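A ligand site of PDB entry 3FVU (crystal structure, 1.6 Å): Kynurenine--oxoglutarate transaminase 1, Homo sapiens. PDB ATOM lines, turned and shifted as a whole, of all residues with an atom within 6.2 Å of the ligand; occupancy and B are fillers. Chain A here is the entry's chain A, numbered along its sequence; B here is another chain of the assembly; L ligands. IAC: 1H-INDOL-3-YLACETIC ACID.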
ATOM      1  N   TRP A  18     -13.825 -15.172  -5.598  1.00  0.00           N
ATOM      2  CA  TRP A  18     -12.688 -15.531  -4.771  1.00  0.00           C
ATOM      3  C   TRP A  18     -11.412 -14.823  -5.196  1.00  0.00           C
ATOM      4  O   TRP A  18     -10.567 -14.493  -4.364  1.00  0.00           O
ATOM      5  CB  TRP A  18     -12.418 -17.043  -4.832  1.00  0.00           C
ATOM      6  CG  TRP A  18     -13.495 -17.904  -4.248  1.00  0.00           C
ATOM      7  CD1 TRP A  18     -14.699 -18.207  -4.814  1.00  0.00           C
ATOM      8  CD2 TRP A  18     -13.456 -18.608  -2.997  1.00  0.00           C
ATOM      9  NE1 TRP A  18     -15.407 -19.052  -4.002  1.00  0.00           N
ATOM     10  CE2 TRP A  18     -14.667 -19.308  -2.871  1.00  0.00           C
ATOM     11  CE3 TRP A  18     -12.527 -18.707  -1.967  1.00  0.00           C
ATOM     12  CZ2 TRP A  18     -14.962 -20.075  -1.763  1.00  0.00           C
ATOM     13  CZ3 TRP A  18     -12.831 -19.471  -0.873  1.00  0.00           C
ATOM     14  CH2 TRP A  18     -14.029 -20.136  -0.783  1.00  0.00           C
ATOM     15  N   GLY A  34      -8.405 -18.156   5.082  1.00  0.00           N
ATOM     16  CA  GLY A  34      -9.364 -18.268   3.969  1.00  0.00           C
ATOM     17  C   GLY A  34      -9.286 -19.606   3.250  1.00  0.00           C
ATOM     18  O   GLY A  34     -10.291 -20.080   2.709  1.00  0.00           O
ATOM     19  N   GLN A  35      -8.097 -20.186   3.202  1.00  0.00           N
ATOM     20  CA  GLN A  35      -7.879 -21.448   2.500  1.00  0.00           C
ATOM     21  C   GLN A  35      -8.640 -22.564   3.199  1.00  0.00           C
ATOM     22  O   GLN A  35      -8.438 -22.825   4.377  1.00  0.00           O
ATOM     23  CB  GLN A  35      -6.383 -21.759   2.479  1.00  0.00           C
ATOM     24  CG  GLN A  35      -5.626 -20.810   1.574  1.00  0.00           C
ATOM     25  CD  GLN A  35      -4.126 -21.033   1.579  1.00  0.00           C
ATOM     26  OE1 GLN A  35      -3.536 -21.415   2.587  1.00  0.00           O
ATOM     27  NE2 GLN A  35      -3.484 -20.777   0.432  1.00  0.00           N
ATOM     28  N   GLY A  36      -9.523 -23.212   2.441  1.00  0.00           N
ATOM     29  CA  GLY A  36     -10.406 -24.263   2.952  1.00  0.00           C
ATOM     30  C   GLY A  36      -9.804 -25.635   2.783  1.00  0.00           C
ATOM     31  O   GLY A  36     -10.421 -26.554   2.196  1.00  0.00           O
ATOM     32  N   PHE A  37      -8.577 -25.781   3.265  1.00  0.00           N
ATOM     33  CA  PHE A  37      -7.837 -27.046   3.215  1.00  0.00           C
ATOM     34  C   PHE A  37      -6.737 -27.037   4.271  1.00  0.00           C
ATOM     35  O   PHE A  37      -6.306 -25.962   4.706  1.00  0.00           O
ATOM     36  CB  PHE A  37      -7.264 -27.333   1.818  1.00  0.00           C
ATOM     37  CG  PHE A  37      -6.433 -26.224   1.219  1.00  0.00           C
ATOM     38  CD1 PHE A  37      -5.056 -26.187   1.403  1.00  0.00           C
ATOM     39  CD2 PHE A  37      -7.030 -25.233   0.465  1.00  0.00           C
ATOM     40  CE1 PHE A  37      -4.302 -25.162   0.822  1.00  0.00           C
ATOM     41  CE2 PHE A  37      -6.300 -24.228  -0.126  1.00  0.00           C
ATOM     42  CZ  PHE A  37      -4.940 -24.180   0.058  1.00  0.00           C
ATOM     43  N   TYR A 101     -16.353 -31.821  -6.534  1.00  0.00           N
ATOM     44  CA  TYR A 101     -16.731 -30.828  -7.511  1.00  0.00           C
ATOM     45  C   TYR A 101     -17.194 -31.500  -8.825  1.00  0.00           C
ATOM     46  O   TYR A 101     -18.257 -31.151  -9.343  1.00  0.00           O
ATOM     47  CB  TYR A 101     -15.561 -29.889  -7.766  1.00  0.00           C
ATOM     48  CG  TYR A 101     -15.924 -28.497  -8.205  1.00  0.00           C
ATOM     49  CD1 TYR A 101     -16.258 -27.529  -7.301  1.00  0.00           C
ATOM     50  CD2 TYR A 101     -15.892 -28.167  -9.562  1.00  0.00           C
ATOM     51  CE1 TYR A 101     -16.552 -26.249  -7.700  1.00  0.00           C
ATOM     52  CE2 TYR A 101     -16.212 -26.894  -9.988  1.00  0.00           C
ATOM     53  CZ  TYR A 101     -16.548 -25.927  -9.062  1.00  0.00           C
ATOM     54  OH  TYR A 101     -16.859 -24.657  -9.473  1.00  0.00           O
ATOM     55  N   PHE A 125     -22.427 -23.316  -0.845  1.00  0.00           N
ATOM     56  CA  PHE A 125     -21.166 -23.526  -1.560  1.00  0.00           C
ATOM     57  C   PHE A 125     -21.349 -22.961  -2.975  1.00  0.00           C
ATOM     58  O   PHE A 125     -22.309 -23.325  -3.667  1.00  0.00           O
ATOM     59  CB  PHE A 125     -20.884 -25.014  -1.590  1.00  0.00           C
ATOM     60  CG  PHE A 125     -19.547 -25.387  -2.155  1.00  0.00           C
ATOM     61  CD1 PHE A 125     -18.372 -25.026  -1.520  1.00  0.00           C
ATOM     62  CD2 PHE A 125     -19.475 -26.164  -3.309  1.00  0.00           C
ATOM     63  CE1 PHE A 125     -17.144 -25.395  -2.032  1.00  0.00           C
ATOM     64  CE2 PHE A 125     -18.247 -26.533  -3.822  1.00  0.00           C
ATOM     65  CZ  PHE A 125     -17.072 -26.152  -3.175  1.00  0.00           C
ATOM     66  N   ASP A 126     -20.484 -22.019  -3.372  1.00  0.00           N
ATOM     67  CA  ASP A 126     -20.911 -21.053  -4.385  1.00  0.00           C
ATOM     68  C   ASP A 126     -21.181 -21.651  -5.769  1.00  0.00           C
ATOM     69  O   ASP A 126     -21.986 -21.088  -6.523  1.00  0.00           O
ATOM     70  CB  ASP A 126     -19.943 -19.865  -4.464  1.00  0.00           C
ATOM     71  CG  ASP A 126     -18.532 -20.291  -4.770  1.00  0.00           C
ATOM     72  OD1 ASP A 126     -17.913 -20.992  -3.942  1.00  0.00           O
ATOM     73  OD2 ASP A 126     -18.029 -19.908  -5.858  1.00  0.00           O
ATOM     74  N   ASN A 185     -20.987 -25.894   4.281  1.00  0.00           N
ATOM     75  CA  ASN A 185     -19.955 -24.890   4.040  1.00  0.00           C
ATOM     76  C   ASN A 185     -20.713 -23.683   3.425  1.00  0.00           C
ATOM     77  O   ASN A 185     -21.390 -23.844   2.405  1.00  0.00           O
ATOM     78  CB  ASN A 185     -18.943 -25.499   3.054  1.00  0.00           C
ATOM     79  CG  ASN A 185     -17.917 -24.467   2.520  1.00  0.00           C
ATOM     80  OD1 ASN A 185     -17.877 -23.301   2.937  1.00  0.00           O
ATOM     81  ND2 ASN A 185     -17.077 -24.943   1.609  1.00  0.00           N
ATOM     82  N   TYR A 216     -18.253 -33.154   4.056  1.00  0.00           N
ATOM     83  CA  TYR A 216     -17.786 -32.959   5.457  1.00  0.00           C
ATOM     84  C   TYR A 216     -18.356 -33.951   6.480  1.00  0.00           C
ATOM     85  O   TYR A 216     -18.289 -33.686   7.687  1.00  0.00           O
ATOM     86  CB  TYR A 216     -18.022 -31.526   5.942  1.00  0.00           C
ATOM     87  CG  TYR A 216     -17.198 -30.528   5.155  1.00  0.00           C
ATOM     88  CD1 TYR A 216     -15.807 -30.517   5.257  1.00  0.00           C
ATOM     89  CD2 TYR A 216     -17.811 -29.654   4.280  1.00  0.00           C
ATOM     90  CE1 TYR A 216     -15.046 -29.618   4.498  1.00  0.00           C
ATOM     91  CE2 TYR A 216     -17.073 -28.773   3.524  1.00  0.00           C
ATOM     92  CZ  TYR A 216     -15.706 -28.760   3.642  1.00  0.00           C
ATOM     93  OH  TYR A 216     -14.994 -27.888   2.846  1.00  0.00           O
ATOM     94  N1  LLP A 247     -18.592 -29.267  -1.723  1.00  0.00           N
ATOM     95  C2  LLP A 247     -18.164 -28.564  -0.615  1.00  0.00           C
ATOM     96  C2' LLP A 247     -19.231 -28.033   0.315  1.00  0.00           C
ATOM     97  C3  LLP A 247     -16.797 -28.385  -0.391  1.00  0.00           C
ATOM     98  O3  LLP A 247     -16.464 -27.717   0.618  1.00  0.00           O
ATOM     99  C4  LLP A 247     -15.848 -28.951  -1.282  1.00  0.00           C
ATOM    100  C4' LLP A 247     -14.444 -29.352  -0.866  1.00  0.00           C
ATOM    101  C5  LLP A 247     -16.326 -29.604  -2.419  1.00  0.00           C
ATOM    102  C6  LLP A 247     -17.683 -29.800  -2.611  1.00  0.00           C
ATOM    103  C5' LLP A 247     -15.404 -30.173  -3.446  1.00  0.00           C
ATOM    104  OP4 LLP A 247     -14.789 -31.419  -3.257  1.00  0.00           O
ATOM    105  P   LLP A 247     -13.454 -31.807  -4.065  1.00  0.00           P
ATOM    106  OP1 LLP A 247     -13.291 -33.254  -3.767  1.00  0.00           O
ATOM    107  OP2 LLP A 247     -12.339 -30.994  -3.446  1.00  0.00           O
ATOM    108  OP3 LLP A 247     -13.690 -31.520  -5.513  1.00  0.00           O
ATOM    109  N   LLP A 247     -11.518 -34.137   1.193  1.00  0.00           N
ATOM    110  CA  LLP A 247     -12.066 -33.637   2.465  1.00  0.00           C
ATOM    111  CB  LLP A 247     -13.456 -32.994   2.277  1.00  0.00           C
ATOM    112  CG  LLP A 247     -13.477 -31.876   1.194  1.00  0.00           C
ATOM    113  CD  LLP A 247     -12.714 -30.623   1.664  1.00  0.00           C
ATOM    114  CE  LLP A 247     -12.618 -29.567   0.559  1.00  0.00           C
ATOM    115  NZ  LLP A 247     -13.972 -28.895   0.293  1.00  0.00           N
ATOM    116  C   LLP A 247     -12.072 -34.722   3.543  1.00  0.00           C
ATOM    117  O   LLP A 247     -11.942 -34.413   4.741  1.00  0.00           O
ATOM    118  N   LYS A 255      -8.141 -34.896  -5.354  1.00  0.00           N
ATOM    119  CA  LYS A 255      -9.301 -34.639  -6.248  1.00  0.00           C
ATOM    120  C   LYS A 255      -9.930 -35.945  -6.727  1.00  0.00           C
ATOM    121  O   LYS A 255     -10.080 -36.192  -7.936  1.00  0.00           O
ATOM    122  CB  LYS A 255      -8.892 -33.757  -7.439  1.00  0.00           C
ATOM    123  CG  LYS A 255      -8.504 -32.355  -7.034  1.00  0.00           C
ATOM    124  CD  LYS A 255      -9.700 -31.466  -6.583  1.00  0.00           C
ATOM    125  CE  LYS A 255     -10.853 -31.369  -7.613  1.00  0.00           C
ATOM    126  NZ  LYS A 255     -11.899 -30.342  -7.228  1.00  0.00           N
ATOM    127  N   PHE A 339     -15.133 -25.022   8.861  1.00  0.00           N
ATOM    128  CA  PHE A 339     -15.380 -23.570   8.911  1.00  0.00           C
ATOM    129  C   PHE A 339     -16.203 -23.050  10.087  1.00  0.00           C
ATOM    130  O   PHE A 339     -17.022 -23.761  10.670  1.00  0.00           O
ATOM    131  CB  PHE A 339     -16.071 -23.124   7.614  1.00  0.00           C
ATOM    132  CG  PHE A 339     -15.400 -23.666   6.396  1.00  0.00           C
ATOM    133  CD1 PHE A 339     -14.149 -23.165   6.004  1.00  0.00           C
ATOM    134  CD2 PHE A 339     -15.977 -24.693   5.656  1.00  0.00           C
ATOM    135  CE1 PHE A 339     -13.496 -23.669   4.873  1.00  0.00           C
ATOM    136  CE2 PHE A 339     -15.332 -25.211   4.514  1.00  0.00           C
ATOM    137  CZ  PHE A 339     -14.086 -24.698   4.126  1.00  0.00           C
ATOM    138  N   ILE A 379     -12.972 -15.187   4.247  1.00  0.00           N
ATOM    139  CA  ILE A 379     -13.739 -15.140   3.012  1.00  0.00           C
ATOM    140  C   ILE A 379     -15.051 -14.442   3.294  1.00  0.00           C
ATOM    141  O   ILE A 379     -15.761 -14.839   4.211  1.00  0.00           O
ATOM    142  CB  ILE A 379     -14.034 -16.560   2.478  1.00  0.00           C
ATOM    143  CG1 ILE A 379     -12.736 -17.349   2.250  1.00  0.00           C
ATOM    144  CG2 ILE A 379     -14.807 -16.533   1.168  1.00  0.00           C
ATOM    145  CD1 ILE A 379     -11.755 -16.655   1.298  1.00  0.00           C
ATOM    146  N   PHE A 384     -21.563 -16.508  -0.857  1.00  0.00           N
ATOM    147  CA  PHE A 384     -22.358 -17.730  -0.699  1.00  0.00           C
ATOM    148  C   PHE A 384     -23.863 -17.416  -0.692  1.00  0.00           C
ATOM    149  O   PHE A 384     -24.669 -18.237  -0.226  1.00  0.00           O
ATOM    150  CB  PHE A 384     -21.977 -18.448   0.594  1.00  0.00           C
ATOM    151  CG  PHE A 384     -20.508 -18.765   0.704  1.00  0.00           C
ATOM    152  CD1 PHE A 384     -19.937 -19.824  -0.026  1.00  0.00           C
ATOM    153  CD2 PHE A 384     -19.700 -18.020   1.533  1.00  0.00           C
ATOM    154  CE1 PHE A 384     -18.573 -20.102   0.074  1.00  0.00           C
ATOM    155  CE2 PHE A 384     -18.330 -18.306   1.655  1.00  0.00           C
ATOM    156  CZ  PHE A 384     -17.773 -19.349   0.916  1.00  0.00           C
ATOM    157  N   ARG A 398     -16.046 -15.823   6.733  1.00  0.00           N
ATOM    158  CA  ARG A 398     -15.740 -17.217   6.987  1.00  0.00           C
ATOM    159  C   ARG A 398     -14.260 -17.436   7.281  1.00  0.00           C
ATOM    160  O   ARG A 398     -13.390 -16.967   6.546  1.00  0.00           O
ATOM    161  CB  ARG A 398     -16.144 -18.100   5.789  1.00  0.00           C
ATOM    162  CG  ARG A 398     -16.166 -19.601   6.075  1.00  0.00           C
ATOM    163  CD  ARG A 398     -16.068 -20.427   4.806  1.00  0.00           C
ATOM    164  NE  ARG A 398     -14.732 -20.406   4.204  1.00  0.00           N
ATOM    165  CZ  ARG A 398     -14.408 -21.056   3.083  1.00  0.00           C
ATOM    166  NH1 ARG A 398     -15.343 -21.738   2.420  1.00  0.00           N
ATOM    167  NH2 ARG A 398     -13.162 -21.011   2.616  1.00  0.00           N
ATOM    168  N   TYR B  63      -4.781 -28.826  -2.673  1.00  0.00           N
ATOM    169  CA  TYR B  63      -5.125 -28.175  -3.925  1.00  0.00           C
ATOM    170  C   TYR B  63      -3.963 -27.389  -4.526  1.00  0.00           C
ATOM    171  O   TYR B  63      -3.197 -26.726  -3.811  1.00  0.00           O
ATOM    172  CB  TYR B  63      -6.222 -27.158  -3.703  1.00  0.00           C
ATOM    173  CG  TYR B  63      -7.583 -27.685  -3.323  1.00  0.00           C
ATOM    174  CD1 TYR B  63      -8.303 -27.075  -2.296  1.00  0.00           C
ATOM    175  CD2 TYR B  63      -8.205 -28.708  -4.056  1.00  0.00           C
ATOM    176  CE1 TYR B  63      -9.592 -27.514  -1.971  1.00  0.00           C
ATOM    177  CE2 TYR B  63      -9.483 -29.127  -3.727  1.00  0.00           C
ATOM    178  CZ  TYR B  63     -10.166 -28.517  -2.709  1.00  0.00           C
ATOM    179  OH  TYR B  63     -11.437 -28.903  -2.358  1.00  0.00           O
ATOM    180  N   VAL B 277     -14.656 -28.997 -12.954  1.00  0.00           N
ATOM    181  CA  VAL B 277     -13.746 -29.752 -12.068  1.00  0.00           C
ATOM    182  C   VAL B 277     -12.993 -28.848 -11.087  1.00  0.00           C
ATOM    183  O   VAL B 277     -12.670 -29.283  -9.967  1.00  0.00           O
ATOM    184  CB  VAL B 277     -12.759 -30.634 -12.801  1.00  0.00           C
ATOM    185  CG1 VAL B 277     -13.485 -31.788 -13.542  1.00  0.00           C
ATOM    186  CG2 VAL B 277     -11.911 -29.827 -13.733  1.00  0.00           C
ATOM    187  N   PHE B 278     -12.739 -27.602 -11.527  1.00  0.00           N
ATOM    188  CA  PHE B 278     -12.041 -26.563 -10.727  1.00  0.00           C
ATOM    189  C   PHE B 278     -10.554 -26.806 -10.566  1.00  0.00           C
ATOM    190  O   PHE B 278      -9.730 -25.947 -10.954  1.00  0.00           O
ATOM    191  CB  PHE B 278     -12.720 -26.243  -9.368  1.00  0.00           C
ATOM    192  CG  PHE B 278     -12.370 -24.870  -8.849  1.00  0.00           C
ATOM    193  CD1 PHE B 278     -13.282 -23.821  -8.933  1.00  0.00           C
ATOM    194  CD2 PHE B 278     -11.100 -24.617  -8.319  1.00  0.00           C
ATOM    195  CE1 PHE B 278     -12.925 -22.539  -8.462  1.00  0.00           C
ATOM    196  CE2 PHE B 278     -10.735 -23.339  -7.848  1.00  0.00           C
ATOM    197  CZ  PHE B 278     -11.653 -22.317  -7.912  1.00  0.00           C
ATOM    198  N   HIS B 279     -10.166 -27.953 -10.015  1.00  0.00           N
ATOM    199  CA  HIS B 279      -8.746 -28.331  -9.899  1.00  0.00           C
ATOM    200  C   HIS B 279      -8.502 -29.645 -10.607  1.00  0.00           C
ATOM    201  O   HIS B 279      -9.364 -30.538 -10.586  1.00  0.00           O
ATOM    202  CB  HIS B 279      -8.273 -28.556  -8.448  1.00  0.00           C
ATOM    203  CG  HIS B 279      -8.975 -27.728  -7.427  1.00  0.00           C
ATOM    204  ND1 HIS B 279      -8.402 -26.598  -6.863  1.00  0.00           N
ATOM    205  CD2 HIS B 279     -10.167 -27.896  -6.809  1.00  0.00           C
ATOM    206  CE1 HIS B 279      -9.245 -26.091  -5.972  1.00  0.00           C
ATOM    207  NE2 HIS B 279     -10.312 -26.871  -5.915  1.00  0.00           N
HETATM  208  C   IAC L   1     -13.730 -24.517  -4.236  1.00  0.00           C
HETATM  209  C1  IAC L   1     -13.435 -25.284  -3.118  1.00  0.00           C
HETATM  210  C2  IAC L   1     -13.259 -26.665  -3.207  1.00  0.00           C
HETATM  211  C3  IAC L   1     -13.397 -27.263  -4.474  1.00  0.00           C
HETATM  212  C4  IAC L   1     -13.696 -26.504  -5.597  1.00  0.00           C
HETATM  213  C5  IAC L   1     -13.880 -25.115  -5.495  1.00  0.00           C
HETATM  214  C7  IAC L   1     -13.369 -24.461  -2.014  1.00  0.00           C
HETATM  215  C8  IAC L   1     -13.626 -23.169  -2.488  1.00  0.00           C
HETATM  216  C17 IAC L   1     -13.063 -24.865  -0.589  1.00  0.00           C
HETATM  217  C18 IAC L   1     -13.452 -23.704   0.288  1.00  0.00           C
HETATM  218  N   IAC L   1     -13.839 -23.233  -3.829  1.00  0.00           N
HETATM  219  O2  IAC L   1     -12.552 -22.908   0.658  1.00  0.00           O
HETATM  220  O3  IAC L   1     -14.688 -23.571   0.542  1.00  0.00           O
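Trp 18 touches the ligand. Gly 36 touches the ligand (CA to O2, 3.4 Å). Tyr 101 touches the ligand. Phe 125 touches the ligand (CZ to C1, 3.7 Å). LLP 247 touches the ligand (C5' to C3, 3.7 Å). Phe 339 touches the ligand. OH of Tyr 63 of chain B touches C2 of the ligand, 3.0 Å away. CG of Phe 278 of chain B touches C5 of the ligand, at 3.7 Å. His 279 of chain B touches the ligand. Hydrophobic or aromatic side chains within 4 Å of the ligand: Trp 18, Tyr 101, Phe 125, Phe 339, Tyr 63 of chain B, Phe 278 of chain B and His 279 of chain B. Of the 20 residues printed, 11 come within 4 Å of the ligand. Along chain A the residues within 4 Å of the ligand span positions 18 to 398.
An oxygen (O3) of the ligand lies within hydrogen-bond range of the side-chain amide nitrogen of Asn 185, at 3.0 Å. An oxygen (O3) of the ligand is in salt-bridge range of the guanidinium group (NH1) of Arg 398 (2.7 Å).
OP2 of LLP 247 is in hydrogen-bond range of the side-chain hydroxyl (OH) of Tyr 63 of chain B (2.5 Å). O3 of LLP 247 is in hydrogen-bond range of ND2 of Asn 185 (3.0 Å). OP3 of LLP 247 sits at hydrogen-bond distance from the backbone NH (N) of Tyr 101 (2.9 Å). The side-chain amino group (NZ) of Lys 255 lies within salt-bridge range of OP3 of LLP 247, 2.7 Å away. O of Asn 185 lies within hydrogen-bond range of N of Phe 125 (3.5 Å). The indole nitrogen (NE1) of Trp 18 is in hydrogen-bond range of the side-chain carboxylate (OD1) of Asp 126, at 3.2 Å. O3 of LLP 247 is in hydrogen-bond range of OH of Tyr 216 (2.7 Å). The side-chain amide oxygen of Asn 185 is in hydrogen-bond range of the guanidinium group of Arg 398 (3.0 Å).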
